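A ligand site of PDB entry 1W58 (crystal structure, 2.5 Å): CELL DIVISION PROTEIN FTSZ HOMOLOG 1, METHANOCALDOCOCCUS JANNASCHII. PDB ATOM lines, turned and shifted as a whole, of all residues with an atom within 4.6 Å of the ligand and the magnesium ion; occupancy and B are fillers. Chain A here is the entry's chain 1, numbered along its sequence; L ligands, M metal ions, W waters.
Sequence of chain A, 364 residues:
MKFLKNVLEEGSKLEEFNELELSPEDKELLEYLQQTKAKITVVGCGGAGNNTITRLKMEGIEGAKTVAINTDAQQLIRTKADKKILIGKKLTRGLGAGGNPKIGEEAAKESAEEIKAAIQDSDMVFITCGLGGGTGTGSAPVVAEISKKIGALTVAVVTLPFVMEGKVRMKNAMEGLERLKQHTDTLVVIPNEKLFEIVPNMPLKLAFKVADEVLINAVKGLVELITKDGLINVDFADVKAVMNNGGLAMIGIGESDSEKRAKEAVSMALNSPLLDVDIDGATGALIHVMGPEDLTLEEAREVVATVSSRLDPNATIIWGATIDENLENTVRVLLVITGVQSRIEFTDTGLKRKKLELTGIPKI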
ATOM      1  N   CYS A  45     -15.891   4.385  18.016  1.00  0.00           N
ATOM      2  CA  CYS A  45     -16.670   5.625  18.042  1.00  0.00           C
ATOM      3  C   CYS A  45     -17.641   5.726  19.221  1.00  0.00           C
ATOM      4  O   CYS A  45     -18.415   4.807  19.482  1.00  0.00           O
ATOM      5  CB  CYS A  45     -17.474   5.779  16.743  1.00  0.00           C
ATOM      6  SG  CYS A  45     -16.619   5.278  15.204  1.00  0.00           S
ATOM      7  N   GLY A  46     -17.615   6.864  19.905  1.00  0.00           N
ATOM      8  CA  GLY A  46     -18.517   7.063  21.022  1.00  0.00           C
ATOM      9  C   GLY A  46     -17.950   6.491  22.296  1.00  0.00           C
ATOM     10  O   GLY A  46     -16.812   6.003  22.317  1.00  0.00           O
ATOM     11  N   GLY A  47     -18.754   6.541  23.353  1.00  0.00           N
ATOM     12  CA  GLY A  47     -18.319   6.024  24.652  1.00  0.00           C
ATOM     13  C   GLY A  47     -17.910   4.565  24.645  1.00  0.00           C
ATOM     14  O   GLY A  47     -16.773   4.256  24.963  1.00  0.00           O
ATOM     15  N   ALA A  48     -18.835   3.668  24.305  1.00  0.00           N
ATOM     16  CA  ALA A  48     -18.535   2.236  24.254  1.00  0.00           C
ATOM     17  C   ALA A  48     -17.357   1.943  23.319  1.00  0.00           C
ATOM     18  O   ALA A  48     -16.470   1.174  23.650  1.00  0.00           O
ATOM     19  CB  ALA A  48     -19.759   1.483  23.790  1.00  0.00           C
ATOM     20  N   ASN A  51     -14.102   2.962  24.905  1.00  0.00           N
ATOM     21  CA  ASN A  51     -13.776   2.035  25.966  1.00  0.00           C
ATOM     22  C   ASN A  51     -13.179   0.742  25.391  1.00  0.00           C
ATOM     23  O   ASN A  51     -12.208   0.225  25.934  1.00  0.00           O
ATOM     24  CB  ASN A  51     -15.014   1.728  26.812  1.00  0.00           C
ATOM     25  CG  ASN A  51     -14.715   0.820  27.988  1.00  0.00           C
ATOM     26  OD1 ASN A  51     -13.738   1.032  28.739  1.00  0.00           O
ATOM     27  ND2 ASN A  51     -15.554  -0.198  28.167  1.00  0.00           N
ATOM     28  N   ASN A  70     -14.550  10.799  19.116  1.00  0.00           N
ATOM     29  CA  ASN A  70     -15.677  11.173  19.936  1.00  0.00           C
ATOM     30  C   ASN A  70     -16.052  12.625  19.747  1.00  0.00           C
ATOM     31  O   ASN A  70     -15.278  13.471  19.285  1.00  0.00           O
ATOM     32  CB  ASN A  70     -15.363  10.913  21.414  1.00  0.00           C
ATOM     33  CG  ASN A  70     -16.560  10.414  22.190  1.00  0.00           C
ATOM     34  OD1 ASN A  70     -16.440   9.540  23.047  1.00  0.00           O
ATOM     35  ND2 ASN A  70     -17.728  10.970  21.905  1.00  0.00           N
ATOM     36  N   THR A  71     -17.281  12.881  20.134  1.00  0.00           N
ATOM     37  CA  THR A  71     -17.892  14.179  20.066  1.00  0.00           C
ATOM     38  C   THR A  71     -17.705  14.784  21.486  1.00  0.00           C
ATOM     39  O   THR A  71     -17.711  16.006  21.646  1.00  0.00           O
ATOM     40  CB  THR A  71     -19.336  13.937  19.731  1.00  0.00           C
ATOM     41  OG1 THR A  71     -19.832  14.962  18.881  1.00  0.00           O
ATOM     42  CG2 THR A  71     -20.102  13.787  20.937  1.00  0.00           C
ATOM     43  N   ASP A  72     -17.503  13.903  22.485  1.00  0.00           N
ATOM     44  CA  ASP A  72     -17.293  14.245  23.911  1.00  0.00           C
ATOM     45  C   ASP A  72     -15.799  14.338  24.282  1.00  0.00           C
ATOM     46  O   ASP A  72     -15.110  13.327  24.361  1.00  0.00           O
ATOM     47  CB  ASP A  72     -17.954  13.186  24.803  1.00  0.00           C
ATOM     48  CG  ASP A  72     -17.893  13.533  26.303  1.00  0.00           C
ATOM     49  OD1 ASP A  72     -16.802  13.757  26.857  1.00  0.00           O
ATOM     50  OD2 ASP A  72     -18.954  13.566  26.936  1.00  0.00           O
ATOM     51  N   GLN A  75     -14.479  12.197  27.493  1.00  0.00           N
ATOM     52  CA  GLN A  75     -14.371  10.763  27.218  1.00  0.00           C
ATOM     53  C   GLN A  75     -13.140  10.487  26.373  1.00  0.00           C
ATOM     54  O   GLN A  75     -12.470   9.475  26.573  1.00  0.00           O
ATOM     55  CB  GLN A  75     -15.617  10.255  26.499  1.00  0.00           C
ATOM     56  CG  GLN A  75     -16.841  10.095  27.387  1.00  0.00           C
ATOM     57  CD  GLN A  75     -17.958   9.309  26.719  1.00  0.00           C
ATOM     58  OE1 GLN A  75     -18.786   8.676  27.391  1.00  0.00           O
ATOM     59  NE2 GLN A  75     -17.999   9.338  25.381  1.00  0.00           N
ATOM     60  N   GLY A  96     -20.186  16.300  23.797  1.00  0.00           N
ATOM     61  CA  GLY A  96     -21.101  15.199  23.524  1.00  0.00           C
ATOM     62  C   GLY A  96     -22.159  15.466  22.461  1.00  0.00           C
ATOM     63  O   GLY A  96     -22.267  16.586  21.911  1.00  0.00           O
ATOM     64  N   ALA A  97     -22.949  14.433  22.144  1.00  0.00           N
ATOM     65  CA  ALA A  97     -24.005  14.567  21.145  1.00  0.00           C
ATOM     66  C   ALA A  97     -25.364  14.320  21.751  1.00  0.00           C
ATOM     67  O   ALA A  97     -26.362  14.291  21.042  1.00  0.00           O
ATOM     68  CB  ALA A  97     -23.781  13.591  20.005  1.00  0.00           C
ATOM     69  N   GLY A  98     -25.393  14.129  23.066  1.00  0.00           N
ATOM     70  CA  GLY A  98     -26.629  13.914  23.801  1.00  0.00           C
ATOM     71  C   GLY A  98     -27.584  12.848  23.289  1.00  0.00           C
ATOM     72  O   GLY A  98     -28.798  13.063  23.305  1.00  0.00           O
ATOM     73  N   GLY A  99     -27.062  11.714  22.851  1.00  0.00           N
ATOM     74  CA  GLY A  99     -27.903  10.639  22.362  1.00  0.00           C
ATOM     75  C   GLY A  99     -28.626  10.885  21.037  1.00  0.00           C
ATOM     76  O   GLY A  99     -29.519  10.119  20.704  1.00  0.00           O
ATOM     77  N   ASN A 100     -28.237  11.890  20.269  1.00  0.00           N
ATOM     78  CA  ASN A 100     -28.906  12.198  18.995  1.00  0.00           C
ATOM     79  C   ASN A 100     -28.089  11.757  17.782  1.00  0.00           C
ATOM     80  O   ASN A 100     -27.067  12.365  17.477  1.00  0.00           O
ATOM     81  CB  ASN A 100     -29.172  13.702  18.901  1.00  0.00           C
ATOM     82  CG  ASN A 100     -30.021  14.082  17.680  1.00  0.00           C
ATOM     83  OD1 ASN A 100     -30.074  13.355  16.684  1.00  0.00           O
ATOM     84  ND2 ASN A 100     -30.654  15.245  17.750  1.00  0.00           N
ATOM     85  N   GLY A 130     -20.930   0.835  20.278  1.00  0.00           N
ATOM     86  CA  GLY A 130     -22.150   0.231  20.788  1.00  0.00           C
ATOM     87  C   GLY A 130     -23.217   1.106  20.164  1.00  0.00           C
ATOM     88  O   GLY A 130     -23.155   2.307  20.326  1.00  0.00           O
ATOM     89  N   LEU A 131     -24.162   0.560  19.405  1.00  0.00           N
ATOM     90  CA  LEU A 131     -25.164   1.429  18.783  1.00  0.00           C
ATOM     91  C   LEU A 131     -26.237   1.736  19.811  1.00  0.00           C
ATOM     92  O   LEU A 131     -26.490   0.925  20.699  1.00  0.00           O
ATOM     93  CB  LEU A 131     -25.791   0.757  17.542  1.00  0.00           C
ATOM     94  CG  LEU A 131     -24.871   0.411  16.355  1.00  0.00           C
ATOM     95  CD1 LEU A 131     -25.570  -0.496  15.342  1.00  0.00           C
ATOM     96  CD2 LEU A 131     -24.401   1.673  15.683  1.00  0.00           C
ATOM     97  N   GLY A 132     -26.869   2.907  19.678  1.00  0.00           N
ATOM     98  CA  GLY A 132     -27.917   3.282  20.600  1.00  0.00           C
ATOM     99  C   GLY A 132     -27.883   4.737  21.010  1.00  0.00           C
ATOM    100  O   GLY A 132     -28.910   5.351  21.249  1.00  0.00           O
ATOM    101  N   GLY A 133     -26.673   5.280  21.122  1.00  0.00           N
ATOM    102  CA  GLY A 133     -26.516   6.671  21.488  1.00  0.00           C
ATOM    103  C   GLY A 133     -26.410   7.568  20.256  1.00  0.00           C
ATOM    104  O   GLY A 133     -26.855   7.195  19.170  1.00  0.00           O
ATOM    105  N   GLY A 134     -25.784   8.727  20.426  1.00  0.00           N
ATOM    106  CA  GLY A 134     -25.680   9.655  19.317  1.00  0.00           C
ATOM    107  C   GLY A 134     -24.396   9.681  18.523  1.00  0.00           C
ATOM    108  O   GLY A 134     -24.466   9.823  17.299  1.00  0.00           O
ATOM    109  N   THR A 135     -23.244   9.530  19.173  1.00  0.00           N
ATOM    110  CA  THR A 135     -21.970   9.608  18.480  1.00  0.00           C
ATOM    111  C   THR A 135     -21.620   8.352  17.669  1.00  0.00           C
ATOM    112  O   THR A 135     -21.241   8.445  16.500  1.00  0.00           O
ATOM    113  CB  THR A 135     -20.838   9.943  19.464  1.00  0.00           C
ATOM    114  OG1 THR A 135     -21.138  11.195  20.086  1.00  0.00           O
ATOM    115  CG2 THR A 135     -19.508  10.129  18.749  1.00  0.00           C
ATOM    116  N   GLY A 136     -21.720   7.187  18.294  1.00  0.00           N
ATOM    117  CA  GLY A 136     -21.403   5.956  17.592  1.00  0.00           C
ATOM    118  C   GLY A 136     -22.382   5.626  16.471  1.00  0.00           C
ATOM    119  O   GLY A 136     -21.963   5.320  15.355  1.00  0.00           O
ATOM    120  N   PRO A 161     -28.304  -2.484  21.768  1.00  0.00           N
ATOM    121  CA  PRO A 161     -28.521  -2.302  23.224  1.00  0.00           C
ATOM    122  C   PRO A 161     -29.398  -3.340  23.921  1.00  0.00           C
ATOM    123  O   PRO A 161     -30.148  -4.083  23.272  1.00  0.00           O
ATOM    124  CB  PRO A 161     -29.152  -0.912  23.293  1.00  0.00           C
ATOM    125  CG  PRO A 161     -30.063  -0.933  22.079  1.00  0.00           C
ATOM    126  CD  PRO A 161     -29.134  -1.526  20.997  1.00  0.00           C
ATOM    127  N   PHE A 162     -29.301  -3.407  25.254  1.00  0.00           N
ATOM    128  CA  PHE A 162     -30.147  -4.332  26.044  1.00  0.00           C
ATOM    129  C   PHE A 162     -31.590  -3.811  25.941  1.00  0.00           C
ATOM    130  O   PHE A 162     -31.764  -2.636  25.651  1.00  0.00           O
ATOM    131  CB  PHE A 162     -29.733  -4.314  27.488  1.00  0.00           C
ATOM    132  CG  PHE A 162     -28.394  -4.916  27.756  1.00  0.00           C
ATOM    133  CD1 PHE A 162     -28.253  -6.296  27.856  1.00  0.00           C
ATOM    134  CD2 PHE A 162     -27.291  -4.125  27.990  1.00  0.00           C
ATOM    135  CE1 PHE A 162     -27.020  -6.875  28.195  1.00  0.00           C
ATOM    136  CE2 PHE A 162     -26.059  -4.683  28.336  1.00  0.00           C
ATOM    137  CZ  PHE A 162     -25.916  -6.056  28.442  1.00  0.00           C
ATOM    138  N   GLU A 165     -32.860  -0.933  28.223  1.00  0.00           N
ATOM    139  CA  GLU A 165     -32.471   0.413  27.893  1.00  0.00           C
ATOM    140  C   GLU A 165     -33.651   1.153  27.245  1.00  0.00           C
ATOM    141  O   GLU A 165     -33.639   2.380  27.152  1.00  0.00           O
ATOM    142  CB  GLU A 165     -31.255   0.419  26.968  1.00  0.00           C
ATOM    143  CG  GLU A 165     -30.009  -0.259  27.552  1.00  0.00           C
ATOM    144  CD  GLU A 165     -28.756   0.079  26.759  1.00  0.00           C
ATOM    145  OE1 GLU A 165     -28.607   1.267  26.428  1.00  0.00           O
ATOM    146  OE2 GLU A 165     -27.928  -0.807  26.481  1.00  0.00           O
ATOM    147  N   ARG A 169     -33.808   3.856  22.438  1.00  0.00           N
ATOM    148  CA  ARG A 169     -32.442   3.487  22.238  1.00  0.00           C
ATOM    149  C   ARG A 169     -32.348   2.383  21.185  1.00  0.00           C
ATOM    150  O   ARG A 169     -31.425   2.389  20.373  1.00  0.00           O
ATOM    151  CB  ARG A 169     -31.795   3.063  23.563  1.00  0.00           C
ATOM    152  CG  ARG A 169     -30.342   3.510  23.711  1.00  0.00           C
ATOM    153  CD  ARG A 169     -30.048   4.121  25.072  1.00  0.00           C
ATOM    154  NE  ARG A 169     -29.576   5.495  24.938  1.00  0.00           N
ATOM    155  CZ  ARG A 169     -28.310   5.873  24.750  1.00  0.00           C
ATOM    156  NH1 ARG A 169     -27.318   4.990  24.671  1.00  0.00           N
ATOM    157  NH2 ARG A 169     -28.027   7.159  24.609  1.00  0.00           N
ATOM    158  N   ASN A 192     -26.637  -7.473  22.486  1.00  0.00           N
ATOM    159  CA  ASN A 192     -26.395  -7.582  23.934  1.00  0.00           C
ATOM    160  C   ASN A 192     -27.487  -8.318  24.721  1.00  0.00           C
ATOM    161  O   ASN A 192     -27.193  -8.945  25.719  1.00  0.00           O
ATOM    162  CB  ASN A 192     -26.232  -6.191  24.555  1.00  0.00           C
ATOM    163  CG  ASN A 192     -24.824  -5.613  24.383  1.00  0.00           C
ATOM    164  OD1 ASN A 192     -24.627  -4.426  24.598  1.00  0.00           O
ATOM    165  ND2 ASN A 192     -23.862  -6.435  24.015  1.00  0.00           N
ATOM    166  N   PHE A 208     -22.760  -4.711  31.271  1.00  0.00           N
ATOM    167  CA  PHE A 208     -21.814  -4.050  30.397  1.00  0.00           C
ATOM    168  C   PHE A 208     -20.381  -4.525  30.560  1.00  0.00           C
ATOM    169  O   PHE A 208     -19.487  -4.149  29.793  1.00  0.00           O
ATOM    170  CB  PHE A 208     -21.889  -2.541  30.602  1.00  0.00           C
ATOM    171  CG  PHE A 208     -23.199  -1.963  30.161  1.00  0.00           C
ATOM    172  CD1 PHE A 208     -23.604  -2.056  28.835  1.00  0.00           C
ATOM    173  CD2 PHE A 208     -24.031  -1.311  31.059  1.00  0.00           C
ATOM    174  CE1 PHE A 208     -24.795  -1.523  28.409  1.00  0.00           C
ATOM    175  CE2 PHE A 208     -25.232  -0.758  30.645  1.00  0.00           C
ATOM    176  CZ  PHE A 208     -25.611  -0.867  29.314  1.00  0.00           C
ATOM    177  N   ALA A 211     -20.572  -7.672  28.190  1.00  0.00           N
ATOM    178  CA  ALA A 211     -20.599  -7.158  26.824  1.00  0.00           C
ATOM    179  C   ALA A 211     -19.213  -6.650  26.439  1.00  0.00           C
ATOM    180  O   ALA A 211     -18.816  -6.786  25.300  1.00  0.00           O
ATOM    181  CB  ALA A 211     -21.631  -6.038  26.693  1.00  0.00           C
ATOM    182  N   ASP A 212     -18.479  -6.073  27.374  1.00  0.00           N
ATOM    183  CA  ASP A 212     -17.149  -5.596  27.061  1.00  0.00           C
ATOM    184  C   ASP A 212     -16.299  -6.792  26.653  1.00  0.00           C
ATOM    185  O   ASP A 212     -15.611  -6.760  25.617  1.00  0.00           O
ATOM    186  CB  ASP A 212     -16.493  -4.931  28.269  1.00  0.00           C
ATOM    187  CG  ASP A 212     -16.983  -3.520  28.490  1.00  0.00           C
ATOM    188  OD1 ASP A 212     -17.774  -3.024  27.670  1.00  0.00           O
ATOM    189  OD2 ASP A 212     -16.565  -2.903  29.481  1.00  0.00           O
ATOM    190  N   LEU A 215     -17.158  -8.145  23.153  1.00  0.00           N
ATOM    191  CA  LEU A 215     -16.645  -7.246  22.120  1.00  0.00           C
ATOM    192  C   LEU A 215     -15.148  -7.431  21.894  1.00  0.00           C
ATOM    193  O   LEU A 215     -14.729  -7.546  20.740  1.00  0.00           O
ATOM    194  CB  LEU A 215     -16.894  -5.784  22.470  1.00  0.00           C
ATOM    195  CG  LEU A 215     -18.055  -5.081  21.781  1.00  0.00           C
ATOM    196  CD1 LEU A 215     -18.263  -3.759  22.480  1.00  0.00           C
ATOM    197  CD2 LEU A 215     -17.781  -4.878  20.305  1.00  0.00           C
HETATM  198  P1  LIG L   1     -23.488  10.227  22.983  1.00  0.00           P
HETATM  199  O1  LIG L   1     -24.669  10.967  22.544  1.00  0.00           O
HETATM  200  O2  LIG L   1     -23.471  10.130  24.444  1.00  0.00           O
HETATM  201  O3  LIG L   1     -22.206  11.035  22.671  1.00  0.00           O
HETATM  202  O4  LIG L   1     -23.442   8.797  22.179  1.00  0.00           O
HETATM  203  P2  LIG L   1     -22.339   7.576  22.344  1.00  0.00           P
HETATM  204  O5  LIG L   1     -22.050   6.993  21.029  1.00  0.00           O
HETATM  205  O6  LIG L   1     -21.124   7.838  23.068  1.00  0.00           O
HETATM  206  C1  LIG L   1     -23.272   6.324  23.190  1.00  0.00           C
HETATM  207  P3  LIG L   1     -22.316   5.283  24.293  1.00  0.00           P
HETATM  208  O7  LIG L   1     -20.977   4.933  23.774  1.00  0.00           O
HETATM  209  O8  LIG L   1     -22.394   5.695  25.697  1.00  0.00           O
HETATM  210  O9  LIG L   1     -23.196   4.002  24.001  1.00  0.00           O
HETATM  211  C2  LIG L   1     -24.563   3.859  24.259  1.00  0.00           C
HETATM  212  C3  LIG L   1     -24.959   2.395  23.947  1.00  0.00           C
HETATM  213  O10 LIG L   1     -23.775   1.513  23.899  1.00  0.00           O
HETATM  214  C4  LIG L   1     -25.893   1.875  25.047  1.00  0.00           C
HETATM  215  O11 LIG L   1     -27.224   1.885  24.515  1.00  0.00           O
HETATM  216  C5  LIG L   1     -25.329   0.505  25.410  1.00  0.00           C
HETATM  217  O12 LIG L   1     -26.033  -0.548  24.784  1.00  0.00           O
HETATM  218  C6  LIG L   1     -23.871   0.481  24.924  1.00  0.00           C
HETATM  219  N1  LIG L   1     -22.915   0.784  26.036  1.00  0.00           N
HETATM  220  C7  LIG L   1     -22.849   1.905  26.872  1.00  0.00           C
HETATM  221  N2  LIG L   1     -21.893   1.890  27.745  1.00  0.00           N
HETATM  222  C8  LIG L   1     -21.228   0.688  27.502  1.00  0.00           C
HETATM  223  C9  LIG L   1     -20.058   0.084  28.149  1.00  0.00           C
HETATM  224  O13 LIG L   1     -19.372   0.526  29.088  1.00  0.00           O
HETATM  225  N3  LIG L   1     -19.729  -1.164  27.593  1.00  0.00           N
HETATM  226  C10 LIG L   1     -20.396  -1.779  26.537  1.00  0.00           C
HETATM  227  N4  LIG L   1     -19.945  -2.974  26.116  1.00  0.00           N
HETATM  228  N5  LIG L   1     -21.473  -1.227  25.938  1.00  0.00           N
HETATM  229  C11 LIG L   1     -21.845  -0.003  26.457  1.00  0.00           C
HETATM  230 MG    MG M   1     -20.806   9.710  24.708  1.00  0.00          MG
HETATM  231  O   HOH W   1     -20.080   3.509  21.252  1.00  0.00           O
HETATM  232  O   HOH W   2     -16.888  -1.114  25.579  1.00  0.00           O
HETATM  233  O   HOH W   3     -21.307  11.893  26.469  1.00  0.00           O
HETATM  234  O   HOH W   4     -19.989   4.799  27.652  1.00  0.00           O
HETATM  235  O   HOH W   5     -25.211  -1.213  22.091  1.00  0.00           O
HETATM  236  O   HOH W   6     -21.483   8.063  26.284  1.00  0.00           O
HETATM  237  O   HOH W   7     -25.984   8.961  25.120  1.00  0.00           O
HETATM  238  O   HOH W   8     -17.751  -0.983  31.017  1.00  0.00           O
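Water W6 binds the magnesium ion, at 2.4 Å.
O6 of the ligand binds the magnesium ion, at 2.5 Å.
The magnesium ion has two donor atoms within binding distance.
Slightly farther from the magnesium ion lies an oxygen (O2) of the ligand (2.7 Å).
Slightly farther from the magnesium ion lies an oxygen (O3) of the ligand (2.8 Å).
Slightly farther from the magnesium ion lies water W3 (2.8 Å).
OE2 of Glu 165 sits at hydrogen-bond distance from N of Phe 162 (3.2 Å).
ND2 of Asn 51 sits at hydrogen-bond distance from OD2 of Asp 212 (3.2 Å).
NE2 of Gln 75 is in hydrogen-bond range of OD1 of Asn 70 (2.8 Å).
OD1 of Asp 72 lies within hydrogen-bond range of N of Gln 75 (2.9 Å).
The backbone carbonyl oxygen (O) of Thr 71 sits at hydrogen-bond distance from the backbone NH (N) of Gly 96, 3.3 Å away.
Gly 46 touches the ligand.
Asn 51 touches the ligand.
Thr 71 touches the ligand (CG2 to O3, 3.9 Å).
Ala 97 touches the ligand (C to O1, 3.5 Å).
Gly 130 touches the ligand.
O of Leu 131 touches C3 of the ligand, at 3.9 Å.
CA of Gly 133 touches C1 of the ligand, at 3.7 Å.
Pro 161 touches the ligand (CA to O12, 3.4 Å).
CD1 of Phe 208 touches C11 of the ligand, 3.6 Å away.
Ala 211 touches the ligand.
Hydrophobic or aromatic side chains that line the ligand: Ala 48, Ala 97, Pro 161, Phe 208 and Ala 211.
Water W6 lies within hydrogen-bond range of O8 of the ligand and OE1 of Gln 75.
Water W3 bridges OD2 of Asp 72 (2.9 Å) and O2 of the ligand (3.4 Å).
Water W7 lies within hydrogen-bond range of the guanidinium group (NH2) of Arg 169 (2.8 Å) and an oxygen (O2) of the ligand (2.9 Å).
Water W8 lies within hydrogen-bond range of OD2 of Asp 212 (2.7 Å) and O13 of the ligand (2.9 Å).
Water W1 lies within hydrogen-bond range of the backbone carbonyl oxygen of Cys 45 (2.8 Å), the backbone NH of Gly 130 (3.0 Å), an oxygen (O7) of the ligand (3.0 Å) and the backbone NH of Ala 48 (3.3 Å).
Water W2 lies within hydrogen-bond range of the side-chain carboxylate (OD1) of Asp 212 (3.0 Å), the backbone carbonyl oxygen (O) of Ala 48 (3.0 Å), the side-chain amide nitrogen (ND2) of Asn 51 (3.1 Å) and a nitrogen (N3) of the ligand (3.5 Å).
Gln 75 touches the magnesium ion (NE2 to MG, 2.9 Å).
Of the 30 residues printed, 1 comes within 4 Å of the magnesium ion.
The nearest printed residue that does not touch the magnesium ion is Gly 47 (4.01 Å).
The side-chain carboxylate (OE1) of Glu 165 is in hydrogen-bond range of an oxygen (O11) of the ligand (2.4 Å).
An oxygen (O1) of the ligand is in hydrogen-bond range of the backbone NH of Gly 99, at 2.5 Å.
N of Ala 48 lies within hydrogen-bond range of O7 of the ligand, at 2.5 Å.
The side-chain carboxylate (OD1) of Asp 212 is in hydrogen-bond range of a nitrogen (N4) of the ligand, 2.7 Å away.
An oxygen (O7) of the ligand sits at hydrogen-bond distance from the backbone NH (N) of Gly 47 (2.8 Å).
The backbone NH (N) of Gly 136 sits at hydrogen-bond distance from an oxygen (O5) of the ligand (2.8 Å).
An oxygen (O4) of the ligand lies within hydrogen-bond range of the backbone NH (N) of Thr 135.
OG1 of Thr 135 lies within hydrogen-bond range of O3 of the ligand (2.8 Å).
An oxygen (O4) of the ligand lies within hydrogen-bond range of the backbone NH (N) of Gly 134, 2.9 Å away.
NH1 of Arg 169 sits close to O11 of the ligand (3.1 Å).
An oxygen (O1) of the ligand sits at hydrogen-bond distance from the backbone NH of Gly 98 (3.3 Å).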
